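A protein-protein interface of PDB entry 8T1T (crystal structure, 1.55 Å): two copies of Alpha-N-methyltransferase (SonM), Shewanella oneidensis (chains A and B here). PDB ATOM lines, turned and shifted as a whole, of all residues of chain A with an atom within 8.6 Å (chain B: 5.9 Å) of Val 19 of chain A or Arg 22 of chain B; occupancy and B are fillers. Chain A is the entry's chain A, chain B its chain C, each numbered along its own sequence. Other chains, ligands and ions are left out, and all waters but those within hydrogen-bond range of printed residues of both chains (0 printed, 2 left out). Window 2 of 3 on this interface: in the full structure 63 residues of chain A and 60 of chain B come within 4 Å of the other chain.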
ATOM      1  N   GLY A   8       5.579  -5.075  -0.170  1.00  0.00           N
ATOM      2  CA  GLY A   8       6.374  -3.862  -0.242  1.00  0.00           C
ATOM      3  C   GLY A   8       7.469  -3.871   0.820  1.00  0.00           C
ATOM      4  O   GLY A   8       7.288  -4.446   1.890  1.00  0.00           O
ATOM      5  N   ALA A  14      15.783  -2.064   5.252  1.00  0.00           N
ATOM      6  CA  ALA A  14      15.726  -3.143   6.234  1.00  0.00           C
ATOM      7  C   ALA A  14      14.579  -2.981   7.231  1.00  0.00           C
ATOM      8  O   ALA A  14      13.919  -3.964   7.570  1.00  0.00           O
ATOM      9  CB  ALA A  14      17.043  -3.267   6.963  1.00  0.00           C
ATOM     10  N   GLY A  15      14.369  -1.762   7.740  1.00  0.00           N
ATOM     11  CA  GLY A  15      13.543  -1.581   8.923  1.00  0.00           C
ATOM     12  C   GLY A  15      12.084  -1.226   8.628  1.00  0.00           C
ATOM     13  O   GLY A  15      11.256  -1.243   9.542  1.00  0.00           O
ATOM     14  N   GLN A  16      11.757  -0.903   7.371  1.00  0.00           N
ATOM     15  CA  GLN A  16      10.460  -0.307   7.076  1.00  0.00           C
ATOM     16  C   GLN A  16       9.511  -1.332   6.456  1.00  0.00           C
ATOM     17  O   GLN A  16       8.369  -1.001   6.142  1.00  0.00           O
ATOM     18  CB  GLN A  16      10.611   0.916   6.169  1.00  0.00           C
ATOM     19  CG  GLN A  16       9.508   1.941   6.376  1.00  0.00           C
ATOM     20  CD  GLN A  16       9.872   3.314   5.867  1.00  0.00           C
ATOM     21  OE1 GLN A  16      10.241   3.484   4.710  1.00  0.00           O
ATOM     22  NE2 GLN A  16       9.775   4.310   6.734  1.00  0.00           N
ATOM     23  N   ILE A  17       9.987  -2.569   6.286  1.00  0.00           N
ATOM     24  CA  ILE A  17       9.148  -3.669   5.835  1.00  0.00           C
ATOM     25  C   ILE A  17       8.319  -4.149   7.025  1.00  0.00           C
ATOM     26  O   ILE A  17       8.787  -4.110   8.162  1.00  0.00           O
ATOM     27  CB  ILE A  17      10.008  -4.793   5.219  1.00  0.00           C
ATOM     28  CG1 ILE A  17       9.158  -5.905   4.600  1.00  0.00           C
ATOM     29  CG2 ILE A  17      11.001  -5.346   6.232  1.00  0.00           C
ATOM     30  CD1 ILE A  17       9.945  -6.879   3.772  1.00  0.00           C
ATOM     31  N   SER A  18       7.086  -4.590   6.756  1.00  0.00           N
ATOM     32  CA  SER A  18       6.252  -5.144   7.813  1.00  0.00           C
ATOM     33  C   SER A  18       6.806  -6.509   8.218  1.00  0.00           C
ATOM     34  O   SER A  18       7.496  -7.158   7.435  1.00  0.00           O
ATOM     35  CB  SER A  18       4.809  -5.224   7.403  1.00  0.00           C
ATOM     36  OG  SER A  18       4.594  -6.347   6.569  1.00  0.00           O
ATOM     37  N   VAL A  19       6.469  -6.935   9.443  1.00  0.00           N
ATOM     38  CA  VAL A  19       6.944  -8.194  10.004  1.00  0.00           C
ATOM     39  C   VAL A  19       6.460  -9.360   9.140  1.00  0.00           C
ATOM     40  O   VAL A  19       7.235 -10.262   8.810  1.00  0.00           O
ATOM     41  CB  VAL A  19       6.477  -8.358  11.464  1.00  0.00           C
ATOM     42  CG1 VAL A  19       6.610  -9.798  11.942  1.00  0.00           C
ATOM     43  CG2 VAL A  19       7.211  -7.408  12.399  1.00  0.00           C
ATOM     44  N   LEU A  20       5.186  -9.320   8.736  1.00  0.00           N
ATOM     45  CA  LEU A  20       4.622 -10.414   7.959  1.00  0.00           C
ATOM     46  C   LEU A  20       5.246 -10.451   6.565  1.00  0.00           C
ATOM     47  O   LEU A  20       5.548 -11.526   6.053  1.00  0.00           O
ATOM     48  CB  LEU A  20       3.098 -10.278   7.886  1.00  0.00           C
ATOM     49  CG  LEU A  20       2.396 -11.328   7.021  1.00  0.00           C
ATOM     50  CD1 LEU A  20       2.537 -12.716   7.618  1.00  0.00           C
ATOM     51  CD2 LEU A  20       0.929 -10.981   6.839  1.00  0.00           C
ATOM     52  N   SER A  21       5.436  -9.279   5.953  1.00  0.00           N
ATOM     53  CA  SER A  21       5.998  -9.198   4.612  1.00  0.00           C
ATOM     54  C   SER A  21       7.413  -9.777   4.592  1.00  0.00           C
ATOM     55  O   SER A  21       7.796 -10.473   3.649  1.00  0.00           O
ATOM     56  CB  SER A  21       5.964  -7.788   4.089  1.00  0.00           C
ATOM     57  OG  SER A  21       4.627  -7.382   3.823  1.00  0.00           O
ATOM     58  N   ARG A  22       8.213  -9.475   5.619  1.00  0.00           N
ATOM     59  CA  ARG A  22       9.558 -10.021   5.705  1.00  0.00           C
ATOM     60  C   ARG A  22       9.482 -11.545   5.747  1.00  0.00           C
ATOM     61  O   ARG A  22      10.271 -12.235   5.108  1.00  0.00           O
ATOM     62  CB  ARG A  22      10.285  -9.457   6.929  1.00  0.00           C
ATOM     63  CG  ARG A  22      11.738  -9.892   7.045  1.00  0.00           C
ATOM     64  CD  ARG A  22      12.415  -9.248   8.242  1.00  0.00           C
ATOM     65  NE  ARG A  22      13.857  -9.449   8.268  1.00  0.00           N
ATOM     66  CZ  ARG A  22      14.463 -10.565   8.657  1.00  0.00           C
ATOM     67  NH1 ARG A  22      13.753 -11.615   9.032  1.00  0.00           N
ATOM     68  NH2 ARG A  22      15.784 -10.627   8.672  1.00  0.00           N
ATOM     69  N   SER A  23       8.523 -12.066   6.519  1.00  0.00           N
ATOM     70  CA  SER A  23       8.311 -13.502   6.625  1.00  0.00           C
ATOM     71  C   SER A  23       7.974 -14.116   5.263  1.00  0.00           C
ATOM     72  O   SER A  23       8.475 -15.185   4.920  1.00  0.00           O
ATOM     73  CB  SER A  23       7.245 -13.800   7.649  1.00  0.00           C
ATOM     74  OG  SER A  23       7.155 -15.192   7.912  1.00  0.00           O
ATOM     75  N   TYR A  24       7.131 -13.443   4.474  1.00  0.00           N
ATOM     76  CA  TYR A  24       6.782 -13.943   3.150  1.00  0.00           C
ATOM     77  C   TYR A  24       8.041 -14.091   2.296  1.00  0.00           C
ATOM     78  O   TYR A  24       8.214 -15.104   1.621  1.00  0.00           O
ATOM     79  CB  TYR A  24       5.741 -13.046   2.470  1.00  0.00           C
ATOM     80  CG  TYR A  24       4.315 -13.455   2.739  1.00  0.00           C
ATOM     81  CD1 TYR A  24       3.825 -14.653   2.248  1.00  0.00           C
ATOM     82  CD2 TYR A  24       3.449 -12.654   3.466  1.00  0.00           C
ATOM     83  CE1 TYR A  24       2.521 -15.053   2.481  1.00  0.00           C
ATOM     84  CE2 TYR A  24       2.140 -13.042   3.713  1.00  0.00           C
ATOM     85  CZ  TYR A  24       1.674 -14.247   3.217  1.00  0.00           C
ATOM     86  OH  TYR A  24       0.384 -14.670   3.440  1.00  0.00           O
ATOM     87  N   ILE A  25       8.933 -13.094   2.366  1.00  0.00           N
ATOM     88  CA  ILE A  25      10.161 -13.119   1.587  1.00  0.00           C
ATOM     89  C   ILE A  25      11.015 -14.306   2.034  1.00  0.00           C
ATOM     90  O   ILE A  25      11.541 -15.047   1.202  1.00  0.00           O
ATOM     91  CB  ILE A  25      10.929 -11.784   1.705  1.00  0.00           C
ATOM     92  CG1 ILE A  25      10.161 -10.625   1.064  1.00  0.00           C
ATOM     93  CG2 ILE A  25      12.322 -11.905   1.110  1.00  0.00           C
ATOM     94  CD1 ILE A  25      10.820  -9.277   1.261  1.00  0.00           C
ATOM     95  N   GLU A  26      11.136 -14.490   3.353  1.00  0.00           N
ATOM     96  CA  GLU A  26      11.996 -15.522   3.912  1.00  0.00           C
ATOM     97  C   GLU A  26      11.557 -16.913   3.446  1.00  0.00           C
ATOM     98  O   GLU A  26      12.396 -17.774   3.186  1.00  0.00           O
ATOM     99  CB  GLU A  26      11.979 -15.421   5.439  1.00  0.00           C
ATOM    100  CG  GLU A  26      12.849 -16.450   6.136  1.00  0.00           C
ATOM    101  CD  GLU A  26      12.829 -16.357   7.654  1.00  0.00           C
ATOM    102  OE1 GLU A  26      12.214 -15.404   8.182  1.00  0.00           O
ATOM    103  OE2 GLU A  26      13.420 -17.243   8.308  1.00  0.00           O
ATOM    104  N   HIS A  27      10.243 -17.139   3.343  1.00  0.00           N
ATOM    105  CA  HIS A  27       9.714 -18.474   3.091  1.00  0.00           C
ATOM    106  C   HIS A  27       9.441 -18.740   1.608  1.00  0.00           C
ATOM    107  O   HIS A  27       9.007 -19.835   1.263  1.00  0.00           O
ATOM    108  CB  HIS A  27       8.459 -18.715   3.938  1.00  0.00           C
ATOM    109  CG  HIS A  27       8.752 -19.000   5.374  1.00  0.00           C
ATOM    110  ND1 HIS A  27       8.502 -18.103   6.391  1.00  0.00           N
ATOM    111  CD2 HIS A  27       9.308 -20.072   5.955  1.00  0.00           C
ATOM    112  CE1 HIS A  27       8.881 -18.633   7.546  1.00  0.00           C
ATOM    113  NE2 HIS A  27       9.372 -19.830   7.304  1.00  0.00           N
ATOM    114  N   PRO A 121      -0.105  -4.747   1.830  1.00  0.00           N
ATOM    115  CA  PRO A 121       0.205  -3.323   1.794  1.00  0.00           C
ATOM    116  C   PRO A 121       1.573  -3.051   2.413  1.00  0.00           C
ATOM    117  O   PRO A 121       2.050  -3.818   3.249  1.00  0.00           O
ATOM    118  CB  PRO A 121      -0.938  -2.678   2.590  1.00  0.00           C
ATOM    119  CG  PRO A 121      -1.452  -3.782   3.489  1.00  0.00           C
ATOM    120  CD  PRO A 121      -1.205  -5.081   2.747  1.00  0.00           C
ATOM    121  N   ALA B  14      -0.327  -7.777  14.832  1.00  0.00           N
ATOM    122  CA  ALA B  14       1.014  -8.316  15.028  1.00  0.00           C
ATOM    123  C   ALA B  14       1.918  -8.139  13.804  1.00  0.00           C
ATOM    124  O   ALA B  14       3.096  -7.825  13.959  1.00  0.00           O
ATOM    125  CB  ALA B  14       0.941  -9.764  15.447  1.00  0.00           C
ATOM    126  N   GLY B  15       1.391  -8.367  12.595  1.00  0.00           N
ATOM    127  CA  GLY B  15       2.245  -8.584  11.438  1.00  0.00           C
ATOM    128  C   GLY B  15       2.436  -7.356  10.556  1.00  0.00           C
ATOM    129  O   GLY B  15       3.270  -7.374   9.651  1.00  0.00           O
ATOM    130  N   GLN B  16       1.653  -6.295  10.788  1.00  0.00           N
ATOM    131  CA  GLN B  16       1.633  -5.168   9.870  1.00  0.00           C
ATOM    132  C   GLN B  16       2.458  -4.000  10.417  1.00  0.00           C
ATOM    133  O   GLN B  16       2.554  -2.960   9.768  1.00  0.00           O
ATOM    134  CB  GLN B  16       0.188  -4.755   9.593  1.00  0.00           C
ATOM    135  CG  GLN B  16      -0.028  -4.211   8.193  1.00  0.00           C
ATOM    136  CD  GLN B  16      -1.479  -4.271   7.782  1.00  0.00           C
ATOM    137  OE1 GLN B  16      -2.361  -3.781   8.481  1.00  0.00           O
ATOM    138  NE2 GLN B  16      -1.737  -4.899   6.645  1.00  0.00           N
ATOM    139  N   ILE B  17       3.073  -4.174  11.593  1.00  0.00           N
ATOM    140  CA  ILE B  17       4.012  -3.191  12.115  1.00  0.00           C
ATOM    141  C   ILE B  17       5.357  -3.352  11.406  1.00  0.00           C
ATOM    142  O   ILE B  17       5.757  -4.464  11.072  1.00  0.00           O
ATOM    143  CB  ILE B  17       4.163  -3.337  13.646  1.00  0.00           C
ATOM    144  CG1 ILE B  17       4.967  -2.184  14.247  1.00  0.00           C
ATOM    145  CG2 ILE B  17       4.770  -4.683  14.011  1.00  0.00           C
ATOM    146  CD1 ILE B  17       4.940  -2.147  15.754  1.00  0.00           C
ATOM    147  N   SER B  18       6.080  -2.241  11.201  1.00  0.00           N
ATOM    148  CA  SER B  18       7.403  -2.322  10.602  1.00  0.00           C
ATOM    149  C   SER B  18       8.383  -2.940  11.597  1.00  0.00           C
ATOM    150  O   SER B  18       8.165  -2.901  12.804  1.00  0.00           O
ATOM    151  CB  SER B  18       7.898  -0.978  10.123  1.00  0.00           C
ATOM    152  OG  SER B  18       8.387  -0.200  11.199  1.00  0.00           O
ATOM    153  N   VAL B  19       9.459  -3.523  11.066  1.00  0.00           N
ATOM    154  CA  VAL B  19      10.480  -4.153  11.884  1.00  0.00           C
ATOM    155  C   VAL B  19      11.059  -3.142  12.877  1.00  0.00           C
ATOM    156  O   VAL B  19      11.202  -3.451  14.057  1.00  0.00           O
ATOM    157  CB  VAL B  19      11.577  -4.772  10.997  1.00  0.00           C
ATOM    158  CG1 VAL B  19      12.790  -5.207  11.802  1.00  0.00           C
ATOM    159  CG2 VAL B  19      11.030  -5.938  10.194  1.00  0.00           C
ATOM    160  N   LEU B  20      11.411  -1.942  12.397  1.00  0.00           N
ATOM    161  CA  LEU B  20      12.033  -0.944  13.254  1.00  0.00           C
ATOM    162  C   LEU B  20      11.036  -0.436  14.297  1.00  0.00           C
ATOM    163  O   LEU B  20      11.400  -0.211  15.446  1.00  0.00           O
ATOM    164  CB  LEU B  20      12.589   0.202  12.405  1.00  0.00           C
ATOM    165  CG  LEU B  20      13.227   1.353  13.181  1.00  0.00           C
ATOM    166  CD1 LEU B  20      14.474   0.889  13.921  1.00  0.00           C
ATOM    167  CD2 LEU B  20      13.555   2.513  12.257  1.00  0.00           C
ATOM    168  N   SER B  21       9.778  -0.240  13.896  1.00  0.00           N
ATOM    169  CA  SER B  21       8.782   0.273  14.825  1.00  0.00           C
ATOM    170  C   SER B  21       8.567  -0.716  15.969  1.00  0.00           C
ATOM    171  O   SER B  21       8.368  -0.301  17.108  1.00  0.00           O
ATOM    172  CB  SER B  21       7.497   0.619  14.124  1.00  0.00           C
ATOM    173  OG  SER B  21       7.683   1.750  13.283  1.00  0.00           O
ATOM    174  N   ARG B  22       8.622  -2.020  15.671  1.00  0.00           N
ATOM    175  CA  ARG B  22       8.475  -3.034  16.702  1.00  0.00           C
ATOM    176  C   ARG B  22       9.641  -2.914  17.683  1.00  0.00           C
ATOM    177  O   ARG B  22       9.454  -3.039  18.888  1.00  0.00           O
ATOM    178  CB  ARG B  22       8.402  -4.440  16.096  1.00  0.00           C
ATOM    179  CG  ARG B  22       8.123  -5.536  17.117  1.00  0.00           C
ATOM    180  CD  ARG B  22       7.808  -6.885  16.489  1.00  0.00           C
ATOM    181  NE  ARG B  22       8.915  -7.441  15.728  1.00  0.00           N
ATOM    182  CZ  ARG B  22       8.926  -8.665  15.206  1.00  0.00           C
ATOM    183  NH1 ARG B  22       7.902  -9.478  15.405  1.00  0.00           N
ATOM    184  NH2 ARG B  22       9.962  -9.075  14.495  1.00  0.00           N
ATOM    185  N   SER B  23      10.839  -2.656  17.142  1.00  0.00           N
ATOM    186  CA  SER B  23      12.043  -2.502  17.944  1.00  0.00           C
ATOM    187  C   SER B  23      11.913  -1.305  18.891  1.00  0.00           C
ATOM    188  O   SER B  23      12.332  -1.377  20.046  1.00  0.00           O
ATOM    189  CB  SER B  23      13.257  -2.373  17.049  1.00  0.00           C
ATOM    190  OG  SER B  23      14.458  -2.418  17.810  1.00  0.00           O
ATOM    191  N   TYR B  24      11.331  -0.201  18.409  1.00  0.00           N
ATOM    192  CA  TYR B  24      11.131   0.983  19.237  1.00  0.00           C
ATOM    193  C   TYR B  24      10.243   0.635  20.431  1.00  0.00           C
ATOM    194  O   TYR B  24      10.514   1.074  21.549  1.00  0.00           O
ATOM    195  CB  TYR B  24      10.534   2.148  18.437  1.00  0.00           C
ATOM    196  CG  TYR B  24      11.551   3.055  17.792  1.00  0.00           C
ATOM    197  CD1 TYR B  24      12.376   3.864  18.560  1.00  0.00           C
ATOM    198  CD2 TYR B  24      11.712   3.090  16.420  1.00  0.00           C
ATOM    199  CE1 TYR B  24      13.326   4.683  17.979  1.00  0.00           C
ATOM    200  CE2 TYR B  24      12.647   3.917  15.821  1.00  0.00           C
ATOM    201  CZ  TYR B  24      13.471   4.703  16.605  1.00  0.00           C
ATOM    202  OH  TYR B  24      14.413   5.521  16.024  1.00  0.00           O
ATOM    203  N   ILE B  25       9.195  -0.163  20.191  1.00  0.00           N
ATOM    204  CA  ILE B  25       8.269  -0.530  21.256  1.00  0.00           C
ATOM    205  C   ILE B  25       9.004  -1.390  22.283  1.00  0.00           C
ATOM    206  O   ILE B  25       8.833  -1.211  23.488  1.00  0.00           O
ATOM    207  CB  ILE B  25       7.026  -1.250  20.693  1.00  0.00           C
ATOM    208  CG1 ILE B  25       6.126  -0.305  19.894  1.00  0.00           C
ATOM    209  CG2 ILE B  25       6.247  -1.933  21.809  1.00  0.00           C
ATOM    210  CD1 ILE B  25       4.993  -0.996  19.163  1.00  0.00           C
ATOM    211  N   GLU B  26       9.810  -2.330  21.791  1.00  0.00           N
ATOM    212  CA  GLU B  26      10.470  -3.307  22.641  1.00  0.00           C
ATOM    213  C   GLU B  26      11.436  -2.618  23.608  1.00  0.00           C
ATOM    214  O   GLU B  26      11.639  -3.094  24.723  1.00  0.00           O
ATOM    215  CB  GLU B  26      11.185  -4.328  21.753  1.00  0.00           C
ATOM    216  CG  GLU B  26      11.690  -5.548  22.495  1.00  0.00           C
ATOM    217  CD  GLU B  26      12.112  -6.690  21.586  1.00  0.00           C
ATOM    218  OE1 GLU B  26      12.040  -6.516  20.351  1.00  0.00           O
ATOM    219  OE2 GLU B  26      12.500  -7.753  22.113  1.00  0.00           O
ATOM    220  N   HIS B  27      12.037  -1.499  23.185  1.00  0.00           N
ATOM    221  CA  HIS B  27      13.103  -0.878  23.959  1.00  0.00           C
ATOM    222  C   HIS B  27      12.630   0.370  24.711  1.00  0.00           C
ATOM    223  O   HIS B  27      13.428   1.008  25.394  1.00  0.00           O
ATOM    224  CB  HIS B  27      14.305  -0.596  23.050  1.00  0.00           C
ATOM    225  CG  HIS B  27      15.097  -1.826  22.742  1.00  0.00           C
ATOM    226  ND1 HIS B  27      15.180  -2.387  21.484  1.00  0.00           N
ATOM    227  CD2 HIS B  27      15.825  -2.614  23.546  1.00  0.00           C
ATOM    228  CE1 HIS B  27      15.948  -3.467  21.537  1.00  0.00           C
ATOM    229  NE2 HIS B  27      16.347  -3.627  22.779  1.00  0.00           N
ATOM    230  N   TRP B  43      -0.981  -8.494  22.544  1.00  0.00           N
ATOM    231  CA  TRP B  43       0.222  -8.555  21.732  1.00  0.00           C
ATOM    232  C   TRP B  43       1.226  -7.508  22.208  1.00  0.00           C
ATOM    233  O   TRP B  43       2.398  -7.812  22.410  1.00  0.00           O
ATOM    234  CB  TRP B  43      -0.136  -8.365  20.253  1.00  0.00           C
ATOM    235  CG  TRP B  43       1.014  -7.937  19.397  1.00  0.00           C
ATOM    236  CD1 TRP B  43       2.032  -8.713  18.930  1.00  0.00           C
ATOM    237  CD2 TRP B  43       1.284  -6.600  18.939  1.00  0.00           C
ATOM    238  NE1 TRP B  43       2.902  -7.961  18.188  1.00  0.00           N
ATOM    239  CE2 TRP B  43       2.474  -6.660  18.183  1.00  0.00           C
ATOM    240  CE3 TRP B  43       0.633  -5.369  19.078  1.00  0.00           C
ATOM    241  CZ2 TRP B  43       3.027  -5.532  17.577  1.00  0.00           C
ATOM    242  CZ3 TRP B  43       1.180  -4.256  18.481  1.00  0.00           C
ATOM    243  CH2 TRP B  43       2.360  -4.341  17.737  1.00  0.00           C
ATOM    244  N   LEU B  47       5.197  -7.526  24.128  1.00  0.00           N
ATOM    245  CA  LEU B  47       6.351  -6.824  23.583  1.00  0.00           C
ATOM    246  C   LEU B  47       7.009  -5.974  24.669  1.00  0.00           C
ATOM    247  O   LEU B  47       8.232  -5.925  24.762  1.00  0.00           O
ATOM    248  CB  LEU B  47       5.910  -5.925  22.423  1.00  0.00           C
ATOM    249  CG  LEU B  47       5.733  -6.597  21.064  1.00  0.00           C
ATOM    250  CD1 LEU B  47       5.470  -5.553  19.990  1.00  0.00           C
ATOM    251  CD2 LEU B  47       6.949  -7.435  20.702  1.00  0.00           C
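N of Val 19 of chain A lies within hydrogen-bond range of O of Ile 17 of chain B, 3.0 Å away. The backbone NH (N) of Val 19 of chain A sits at hydrogen-bond distance from the backbone carbonyl oxygen (O) of Gly 15 of chain B. The backbone carbonyl oxygen (O) of Gly 15 of chain A lies within hydrogen-bond range of the backbone NH (N) of Leu 20 of chain B (2.9 Å). O of Gly 15 of chain A is in hydrogen-bond range of N of Val 19 of chain B (3.3 Å). The backbone NH of Val 19 of chain B is in hydrogen-bond range of the backbone carbonyl oxygen of Ile 17 of chain A, at 3.0 Å. The backbone NH (N) of Leu 20 of chain A is in hydrogen-bond range of the backbone carbonyl oxygen (O) of Gly 15 of chain B, 2.9 Å away. The side-chain hydroxyl of Ser 18 of chain B lies close to the backbone carbonyl oxygen of Gly 15 of chain A, at 3.5 Å.
OG of Ser 18 of chain A lies within hydrogen-bond range of OG of Ser 21 of chain A (2.9 Å). The side-chain hydroxyl of Ser 18 of chain B is in hydrogen-bond range of the side-chain hydroxyl of Ser 21 of chain B (2.9 Å).
O of Ile 17 of chain A touches CA of Ser 18 of chain B, at 3.3 Å. Ser 18 of chain A touches Gly 15 of chain B (CB to O, 3.5 Å). O of Gln 16 of chain B touches CB of Ser 18 of chain A, 3.98 Å away. Ser 18 of chain A touches Ile 17 of chain B. CZ of Arg 22 of chain B touches CG2 of Val 19 of chain A, 3.5 Å away. NE2 of Gln 16 of chain B touches CG of Pro 121 of chain A, at 3.4 Å.
Of the printed residues of chain B, Ile 17 of chain A touches Ser 18 (3.3 Å) and Val 19 (3.0 Å). Of chain B, only Gly 15, Ile 17 and Arg 22 come within 4 Å of Val 19 of chain A. Printed residues of chain B within 4 Å of Pro 121 of chain A: Gln 16. Of the printed residues of chain A, Val 19 of chain B touches Gly 15 (3.3 Å) and Ile 17 (3.0 Å). Of the printed residues of chain A, Arg 22 of chain B touches Val 19 (3.5 Å). Ser 23 of chain B touches none of the printed residues of chain A. Leu 47 of chain B touches none of the printed residues of chain A. The nearest printed residue of chain A that does not touch Arg 22 of chain B is Gly 15 of chain A (6.7 Å).
Printed residues of chain B that touch a printed residue of chain A: Gly 15, Gln 16, Ile 17, Ser 18, Val 19, Leu 20 and Arg 22. Hydrophobic or aromatic side chains of chain B that line the printed part of chain A: Ile 17, Val 19 and Leu 20. Among the printed residues, no Asp or Glu carboxylate lies within 4 Å of a Lys or Arg side-chain nitrogen of the other chain.
Gly 15 of chain A touches Val 19 of chain B, and with the chains exchanged Val 19 of chain A touches Gly 15 of chain B. Ile 17 of chain A touches Ser 18 of chain B, and with the chains exchanged Ser 18 of chain A touches Ile 17 of chain B. Ile 17 of chain A touches Val 19 of chain B, and with the chains exchanged Val 19 of chain A touches Ile 17 of chain B. Val 19 of chain A touches Arg 22 of chain B, but with the chains exchanged Arg 22 of chain A does not touch Val 19 of chain B (4.1 Å). Positions printed for both chains: 14, 15, 16, 17, 18, 19, 20, 21, 22, 23, 24, 25, 26 and 27. Of the 13 pairs that touch across the chains among the printed residues, 10 have their exchanged pair printed and touching as well.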
